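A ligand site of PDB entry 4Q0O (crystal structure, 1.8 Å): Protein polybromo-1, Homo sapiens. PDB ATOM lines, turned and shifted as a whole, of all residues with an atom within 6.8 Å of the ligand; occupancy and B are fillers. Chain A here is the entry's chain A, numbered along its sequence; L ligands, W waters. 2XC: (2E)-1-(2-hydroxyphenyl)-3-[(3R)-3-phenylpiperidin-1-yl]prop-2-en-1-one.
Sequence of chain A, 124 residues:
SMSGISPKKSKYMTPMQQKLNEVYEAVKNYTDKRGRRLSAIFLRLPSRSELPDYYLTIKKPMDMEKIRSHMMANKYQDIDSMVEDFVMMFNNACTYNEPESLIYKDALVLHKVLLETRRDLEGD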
ATOM      1  N   ILE A  41     -23.190 -13.351 -12.966  1.00  0.00           N
ATOM      2  CA  ILE A  41     -23.263 -13.224 -14.430  1.00  0.00           C
ATOM      3  C   ILE A  41     -23.647 -14.541 -15.090  1.00  0.00           C
ATOM      4  O   ILE A  41     -24.070 -14.585 -16.239  1.00  0.00           O
ATOM      5  CB  ILE A  41     -21.891 -12.680 -14.997  1.00  0.00           C
ATOM      6  CG1 ILE A  41     -22.117 -11.907 -16.299  1.00  0.00           C
ATOM      7  CG2 ILE A  41     -20.843 -13.781 -15.193  1.00  0.00           C
ATOM      8  CD1 ILE A  41     -20.995 -10.950 -16.641  1.00  0.00           C
ATOM      9  N   PHE A  42     -23.568 -15.619 -14.317  1.00  0.00           N
ATOM     10  CA  PHE A  42     -23.786 -17.000 -14.802  1.00  0.00           C
ATOM     11  C   PHE A  42     -25.218 -17.458 -14.582  1.00  0.00           C
ATOM     12  O   PHE A  42     -25.621 -18.521 -15.104  1.00  0.00           O
ATOM     13  CB  PHE A  42     -22.821 -18.015 -14.178  1.00  0.00           C
ATOM     14  CG  PHE A  42     -21.395 -17.794 -14.564  1.00  0.00           C
ATOM     15  CD1 PHE A  42     -20.925 -18.134 -15.820  1.00  0.00           C
ATOM     16  CD2 PHE A  42     -20.498 -17.250 -13.653  1.00  0.00           C
ATOM     17  CE1 PHE A  42     -19.617 -17.915 -16.142  1.00  0.00           C
ATOM     18  CE2 PHE A  42     -19.188 -16.977 -13.996  1.00  0.00           C
ATOM     19  CZ  PHE A  42     -18.755 -17.333 -15.247  1.00  0.00           C
ATOM     20  N   LEU A  43     -26.012 -16.696 -13.857  1.00  0.00           N
ATOM     21  CA  LEU A  43     -27.373 -17.187 -13.552  1.00  0.00           C
ATOM     22  C   LEU A  43     -28.237 -17.238 -14.787  1.00  0.00           C
ATOM     23  O   LEU A  43     -28.962 -18.195 -14.995  1.00  0.00           O
ATOM     24  CB  LEU A  43     -28.088 -16.355 -12.485  1.00  0.00           C
ATOM     25  CG  LEU A  43     -27.502 -16.131 -11.078  1.00  0.00           C
ATOM     26  CD1 LEU A  43     -28.563 -15.471 -10.176  1.00  0.00           C
ATOM     27  CD2 LEU A  43     -27.011 -17.396 -10.417  1.00  0.00           C
ATOM     28  N   ARG A  44     -28.199 -16.196 -15.610  1.00  0.00           N
ATOM     29  CA  ARG A  44     -29.023 -16.133 -16.793  1.00  0.00           C
ATOM     30  C   ARG A  44     -28.236 -15.568 -17.992  1.00  0.00           C
ATOM     31  O   ARG A  44     -27.756 -14.423 -17.997  1.00  0.00           O
ATOM     32  CB  ARG A  44     -30.257 -15.273 -16.499  1.00  0.00           C
ATOM     33  CG  ARG A  44     -31.343 -15.405 -17.528  1.00  0.00           C
ATOM     34  CD  ARG A  44     -32.054 -16.779 -17.549  1.00  0.00           C
ATOM     35  NE  ARG A  44     -33.045 -16.792 -18.610  1.00  0.00           N
ATOM     36  CZ  ARG A  44     -32.942 -17.355 -19.815  1.00  0.00           C
ATOM     37  NH1 ARG A  44     -31.861 -18.026 -20.223  1.00  0.00           N
ATOM     38  NH2 ARG A  44     -33.973 -17.250 -20.653  1.00  0.00           N
ATOM     39  N   LEU A  45     -28.057 -16.405 -19.009  1.00  0.00           N
ATOM     40  CA  LEU A  45     -27.363 -16.034 -20.181  1.00  0.00           C
ATOM     41  C   LEU A  45     -28.229 -14.996 -20.902  1.00  0.00           C
ATOM     42  O   LEU A  45     -29.466 -15.114 -20.898  1.00  0.00           O
ATOM     43  CB  LEU A  45     -27.181 -17.257 -21.049  1.00  0.00           C
ATOM     44  CG  LEU A  45     -26.348 -17.133 -22.315  1.00  0.00           C
ATOM     45  CD1 LEU A  45     -24.890 -16.819 -21.998  1.00  0.00           C
ATOM     46  CD2 LEU A  45     -26.443 -18.472 -23.043  1.00  0.00           C
ATOM     47  N   PRO A  46     -27.586 -13.939 -21.444  1.00  0.00           N
ATOM     48  CA  PRO A  46     -28.326 -13.014 -22.296  1.00  0.00           C
ATOM     49  C   PRO A  46     -28.926 -13.676 -23.530  1.00  0.00           C
ATOM     50  O   PRO A  46     -28.573 -14.841 -23.883  1.00  0.00           O
ATOM     51  CB  PRO A  46     -27.254 -11.966 -22.688  1.00  0.00           C
ATOM     52  CG  PRO A  46     -26.279 -12.003 -21.561  1.00  0.00           C
ATOM     53  CD  PRO A  46     -26.204 -13.470 -21.206  1.00  0.00           C
ATOM     54  N   LEU A  51     -26.548 -11.281 -27.545  1.00  0.00           N
ATOM     55  CA  LEU A  51     -25.217 -11.801 -27.793  1.00  0.00           C
ATOM     56  C   LEU A  51     -25.326 -12.769 -28.995  1.00  0.00           C
ATOM     57  O   LEU A  51     -25.238 -13.983 -28.802  1.00  0.00           O
ATOM     58  CB  LEU A  51     -24.673 -12.591 -26.560  1.00  0.00           C
ATOM     59  CG  LEU A  51     -24.272 -11.897 -25.250  1.00  0.00           C
ATOM     60  CD1 LEU A  51     -23.878 -12.999 -24.239  1.00  0.00           C
ATOM     61  CD2 LEU A  51     -23.157 -10.906 -25.469  1.00  0.00           C
ATOM     62  N   TYR A  54     -22.549 -15.434 -29.540  1.00  0.00           N
ATOM     63  CA  TYR A  54     -22.528 -16.486 -28.531  1.00  0.00           C
ATOM     64  C   TYR A  54     -23.266 -17.688 -29.004  1.00  0.00           C
ATOM     65  O   TYR A  54     -22.777 -18.787 -28.985  1.00  0.00           O
ATOM     66  CB  TYR A  54     -23.119 -15.979 -27.190  1.00  0.00           C
ATOM     67  CG  TYR A  54     -22.815 -16.851 -26.051  1.00  0.00           C
ATOM     68  CD1 TYR A  54     -21.793 -16.538 -25.163  1.00  0.00           C
ATOM     69  CD2 TYR A  54     -23.531 -18.020 -25.834  1.00  0.00           C
ATOM     70  CE1 TYR A  54     -21.482 -17.372 -24.085  1.00  0.00           C
ATOM     71  CE2 TYR A  54     -23.238 -18.864 -24.799  1.00  0.00           C
ATOM     72  CZ  TYR A  54     -22.205 -18.556 -23.930  1.00  0.00           C
ATOM     73  OH  TYR A  54     -21.996 -19.431 -22.931  1.00  0.00           O
ATOM     74  N   ILE A  58     -21.468 -21.150 -29.570  1.00  0.00           N
ATOM     75  CA  ILE A  58     -21.620 -22.094 -28.443  1.00  0.00           C
ATOM     76  C   ILE A  58     -22.756 -23.063 -28.767  1.00  0.00           C
ATOM     77  O   ILE A  58     -23.900 -22.662 -28.955  1.00  0.00           O
ATOM     78  CB  ILE A  58     -21.854 -21.320 -27.122  1.00  0.00           C
ATOM     79  CG1 ILE A  58     -20.660 -20.359 -26.834  1.00  0.00           C
ATOM     80  CG2 ILE A  58     -22.092 -22.301 -25.970  1.00  0.00           C
ATOM     81  CD1 ILE A  58     -19.282 -21.033 -26.752  1.00  0.00           C
ATOM     82  N   MET A  62     -25.868 -22.828 -21.740  1.00  0.00           N
ATOM     83  CA  MET A  62     -26.230 -23.304 -20.405  1.00  0.00           C
ATOM     84  C   MET A  62     -26.082 -22.144 -19.416  1.00  0.00           C
ATOM     85  O   MET A  62     -25.151 -21.376 -19.506  1.00  0.00           O
ATOM     86  CB  MET A  62     -25.283 -24.424 -19.983  1.00  0.00           C
ATOM     87  CG  MET A  62     -25.584 -25.106 -18.648  1.00  0.00           C
ATOM     88  SD  MET A  62     -27.215 -25.876 -18.532  1.00  0.00           S
ATOM     89  CE  MET A  62     -27.086 -27.036 -19.943  1.00  0.00           C
ATOM     90  N   ASP A  63     -27.015 -22.038 -18.498  1.00  0.00           N
ATOM     91  CA  ASP A  63     -26.878 -21.086 -17.396  1.00  0.00           C
ATOM     92  C   ASP A  63     -27.341 -21.711 -16.105  1.00  0.00           C
ATOM     93  O   ASP A  63     -27.908 -22.849 -16.100  1.00  0.00           O
ATOM     94  CB  ASP A  63     -27.507 -19.718 -17.731  1.00  0.00           C
ATOM     95  CG  ASP A  63     -28.971 -19.760 -18.000  1.00  0.00           C
ATOM     96  OD1 ASP A  63     -29.657 -20.650 -17.455  1.00  0.00           O
ATOM     97  OD2 ASP A  63     -29.455 -18.855 -18.762  1.00  0.00           O
ATOM     98  N   MET A  64     -27.138 -21.008 -14.986  1.00  0.00           N
ATOM     99  CA  MET A  64     -27.476 -21.618 -13.737  1.00  0.00           C
ATOM    100  C   MET A  64     -28.972 -21.710 -13.524  1.00  0.00           C
ATOM    101  O   MET A  64     -29.424 -22.644 -12.876  1.00  0.00           O
ATOM    102  CB  MET A  64     -26.786 -20.950 -12.560  1.00  0.00           C
ATOM    103  CG  MET A  64     -25.287 -21.211 -12.575  1.00  0.00           C
ATOM    104  SD  MET A  64     -24.264 -20.517 -11.249  1.00  0.00           S
ATOM    105  CE  MET A  64     -25.130 -21.349  -9.878  1.00  0.00           C
ATOM    106  N   MET A  89     -21.280 -25.339 -18.838  1.00  0.00           N
ATOM    107  CA  MET A  89     -21.372 -23.892 -18.731  1.00  0.00           C
ATOM    108  C   MET A  89     -19.985 -23.242 -18.618  1.00  0.00           C
ATOM    109  O   MET A  89     -19.757 -22.197 -19.227  1.00  0.00           O
ATOM    110  CB  MET A  89     -22.259 -23.524 -17.506  1.00  0.00           C
ATOM    111  CG  MET A  89     -22.550 -22.039 -17.336  1.00  0.00           C
ATOM    112  SD  MET A  89     -23.506 -21.716 -15.812  1.00  0.00           S
ATOM    113  CE  MET A  89     -22.231 -21.994 -14.601  1.00  0.00           C
ATOM    114  N   PHE A  90     -19.134 -23.783 -17.749  1.00  0.00           N
ATOM    115  CA  PHE A  90     -17.819 -23.206 -17.519  1.00  0.00           C
ATOM    116  C   PHE A  90     -16.946 -23.317 -18.757  1.00  0.00           C
ATOM    117  O   PHE A  90     -16.226 -22.379 -19.131  1.00  0.00           O
ATOM    118  CB  PHE A  90     -17.134 -23.849 -16.328  1.00  0.00           C
ATOM    119  CG  PHE A  90     -17.835 -23.587 -15.014  1.00  0.00           C
ATOM    120  CD1 PHE A  90     -18.314 -22.312 -14.739  1.00  0.00           C
ATOM    121  CD2 PHE A  90     -18.004 -24.596 -14.076  1.00  0.00           C
ATOM    122  CE1 PHE A  90     -18.972 -22.052 -13.536  1.00  0.00           C
ATOM    123  CE2 PHE A  90     -18.661 -24.327 -12.869  1.00  0.00           C
ATOM    124  CZ  PHE A  90     -19.153 -23.060 -12.620  1.00  0.00           C
ATOM    125  N   ASN A  91     -17.088 -24.419 -19.440  1.00  0.00           N
ATOM    126  CA  ASN A  91     -16.346 -24.575 -20.690  1.00  0.00           C
ATOM    127  C   ASN A  91     -16.864 -23.633 -21.779  1.00  0.00           C
ATOM    128  O   ASN A  91     -16.100 -23.060 -22.525  1.00  0.00           O
ATOM    129  CB  ASN A  91     -16.395 -26.016 -21.125  1.00  0.00           C
ATOM    130  CG  ASN A  91     -15.175 -26.374 -21.906  1.00  0.00           C
ATOM    131  OD1 ASN A  91     -13.989 -26.321 -21.409  1.00  0.00           O
ATOM    132  ND2 ASN A  91     -15.424 -26.671 -23.151  1.00  0.00           N
ATOM    133  N   ASN A  92     -18.172 -23.430 -21.828  1.00  0.00           N
ATOM    134  CA  ASN A  92     -18.724 -22.431 -22.733  1.00  0.00           C
ATOM    135  C   ASN A  92     -18.171 -21.048 -22.390  1.00  0.00           C
ATOM    136  O   ASN A  92     -17.808 -20.306 -23.282  1.00  0.00           O
ATOM    137  CB  ASN A  92     -20.254 -22.376 -22.673  1.00  0.00           C
ATOM    138  CG  ASN A  92     -20.940 -23.642 -23.201  1.00  0.00           C
ATOM    139  OD1 ASN A  92     -20.329 -24.476 -23.855  1.00  0.00           O
ATOM    140  ND2 ASN A  92     -22.196 -23.806 -22.875  1.00  0.00           N
ATOM    141  N   ALA A  93     -18.114 -20.703 -21.086  1.00  0.00           N
ATOM    142  CA  ALA A  93     -17.605 -19.402 -20.763  1.00  0.00           C
ATOM    143  C   ALA A  93     -16.118 -19.240 -21.171  1.00  0.00           C
ATOM    144  O   ALA A  93     -15.701 -18.170 -21.611  1.00  0.00           O
ATOM    145  CB  ALA A  93     -17.774 -19.155 -19.261  1.00  0.00           C
ATOM    146  N   CYS A  94     -15.339 -20.290 -20.937  1.00  0.00           N
ATOM    147  CA  CYS A  94     -13.902 -20.277 -21.245  1.00  0.00           C
ATOM    148  C   CYS A  94     -13.698 -20.416 -22.753  1.00  0.00           C
ATOM    149  O   CYS A  94     -12.687 -19.959 -23.249  1.00  0.00           O
ATOM    150  CB  CYS A  94     -13.148 -21.341 -20.488  1.00  0.00           C
ATOM    151  SG  CYS A  94     -13.103 -21.044 -18.713  1.00  0.00           S
ATOM    152  N   TYR A  96     -16.009 -18.826 -25.115  1.00  0.00           N
ATOM    153  CA  TYR A  96     -16.423 -17.553 -25.662  1.00  0.00           C
ATOM    154  C   TYR A  96     -15.521 -16.384 -25.293  1.00  0.00           C
ATOM    155  O   TYR A  96     -15.240 -15.504 -26.104  1.00  0.00           O
ATOM    156  CB  TYR A  96     -17.851 -17.263 -25.141  1.00  0.00           C
ATOM    157  CG  TYR A  96     -18.428 -16.002 -25.728  1.00  0.00           C
ATOM    158  CD1 TYR A  96     -18.837 -15.972 -27.065  1.00  0.00           C
ATOM    159  CD2 TYR A  96     -18.521 -14.840 -24.990  1.00  0.00           C
ATOM    160  CE1 TYR A  96     -19.371 -14.844 -27.606  1.00  0.00           C
ATOM    161  CE2 TYR A  96     -19.050 -13.679 -25.531  1.00  0.00           C
ATOM    162  CZ  TYR A  96     -19.475 -13.701 -26.844  1.00  0.00           C
ATOM    163  OH  TYR A  96     -19.994 -12.591 -27.403  1.00  0.00           O
ATOM    164  N   ASN A  97     -15.122 -16.344 -24.007  1.00  0.00           N
ATOM    165  CA  ASN A  97     -14.400 -15.215 -23.465  1.00  0.00           C
ATOM    166  C   ASN A  97     -12.882 -15.525 -23.531  1.00  0.00           C
ATOM    167  O   ASN A  97     -12.485 -16.724 -23.469  1.00  0.00           O
ATOM    168  CB  ASN A  97     -14.836 -14.974 -22.016  1.00  0.00           C
ATOM    169  CG  ASN A  97     -16.324 -14.726 -21.905  1.00  0.00           C
ATOM    170  OD1 ASN A  97     -16.790 -13.643 -22.262  1.00  0.00           O
ATOM    171  ND2 ASN A  97     -17.099 -15.760 -21.563  1.00  0.00           N
ATOM    172  N   ILE A 103     -14.463 -12.838 -16.530  1.00  0.00           N
ATOM    173  CA  ILE A 103     -15.458 -13.909 -16.630  1.00  0.00           C
ATOM    174  C   ILE A 103     -14.789 -15.292 -16.763  1.00  0.00           C
ATOM    175  O   ILE A 103     -15.233 -16.249 -16.167  1.00  0.00           O
ATOM    176  CB  ILE A 103     -16.530 -13.656 -17.691  1.00  0.00           C
ATOM    177  CG1 ILE A 103     -17.664 -14.669 -17.584  1.00  0.00           C
ATOM    178  CG2 ILE A 103     -15.956 -13.678 -19.098  1.00  0.00           C
ATOM    179  CD1 ILE A 103     -18.847 -14.366 -18.508  1.00  0.00           C
HETATM  180  CAS 2XC L   1     -22.634  -8.265 -19.641  1.00  0.00           C
HETATM  181  CAT 2XC L   1     -23.686  -7.725 -18.896  1.00  0.00           C
HETATM  182  CAU 2XC L   1     -24.650  -8.546 -18.366  1.00  0.00           C
HETATM  183  CAV 2XC L   1     -24.666  -9.931 -18.577  1.00  0.00           C
HETATM  184  CAW 2XC L   1     -23.598 -10.479 -19.337  1.00  0.00           C
HETATM  185  CAR 2XC L   1     -22.583  -9.619 -19.855  1.00  0.00           C
HETATM  186  CAP 2XC L   1     -21.451  -9.978 -20.640  1.00  0.00           C
HETATM  187  CAQ 2XC L   1     -21.551 -11.373 -20.933  1.00  0.00           C
HETATM  188  CAO 2XC L   1     -20.111  -9.664 -19.907  1.00  0.00           C
HETATM  189  CAN 2XC L   1     -19.061 -10.716 -20.231  1.00  0.00           C
HETATM  190  CAM 2XC L   1     -19.209 -11.121 -21.727  1.00  0.00           C
HETATM  191  NAL 2XC L   1     -20.428 -11.977 -21.745  1.00  0.00           N
HETATM  192  CAK 2XC L   1     -20.225 -13.261 -21.482  1.00  0.00           C
HETATM  193  CAI 2XC L   1     -21.185 -14.191 -20.721  1.00  0.00           C
HETATM  194  CAH 2XC L   1     -20.906 -15.674 -20.600  1.00  0.00           C
HETATM  195  OAJ 2XC L   1     -19.960 -16.200 -21.228  1.00  0.00           O
HETATM  196  CAE 2XC L   1     -21.821 -16.479 -19.910  1.00  0.00           C
HETATM  197  CAD 2XC L   1     -22.917 -15.967 -19.157  1.00  0.00           C
HETATM  198  CAC 2XC L   1     -23.787 -16.848 -18.518  1.00  0.00           C
HETATM  199  CAB 2XC L   1     -23.642 -18.226 -18.654  1.00  0.00           C
HETATM  200  CAA 2XC L   1     -22.586 -18.727 -19.436  1.00  0.00           C
HETATM  201  CAF 2XC L   1     -21.703 -17.853 -20.040  1.00  0.00           C
HETATM  202  OAG 2XC L   1     -20.665 -18.370 -20.827  1.00  0.00           O
HETATM  203  O   HOH W   1     -25.495 -13.002 -17.757  1.00  0.00           O
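The side-chain hydroxyl (OH) of Tyr 54 sits at hydrogen-bond distance from an oxygen (OAG) of the ligand (2.7 Å). An oxygen (OAJ) of the ligand sits at hydrogen-bond distance from the side-chain amide nitrogen (ND2) of Asn 97 (2.9 Å). The backbone NH (N) of Ala 93 lies close to an oxygen (OAG) of the ligand, 3.5 Å away.
N of Met 64 sits close to SD of Met 89, 3.8 Å away. The backbone carbonyl oxygen (O) of Phe 42 sits at hydrogen-bond distance from the backbone NH (N) of Met 64, 2.9 Å away. The backbone carbonyl oxygen (O) of Ala 93 is in hydrogen-bond range of the side-chain amide nitrogen (ND2) of Asn 97, 2.8 Å away. The backbone NH (N) of Leu 45 lies within hydrogen-bond range of the side-chain carboxylate (OD2) of Asp 63, at 2.8 Å.
Residues that only touch the ligand: Ile 103 (3.2 Å), Ile 41 (3.2 Å), Leu 45 (3.6 Å), Met 62 (3.6 Å), Phe 42 (3.7 Å), Pro 46 (3.8 Å), Met 89 (3.9 Å) and Asn 92 (3.98 Å). Hydrophobic or aromatic side chains that line the ligand: Ile 41, Phe 42, Leu 45, Pro 46, Tyr 54, Met 89, Ala 93 and Ile 103. Of the 21 residues printed, 11 come within 4 Å of the ligand.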
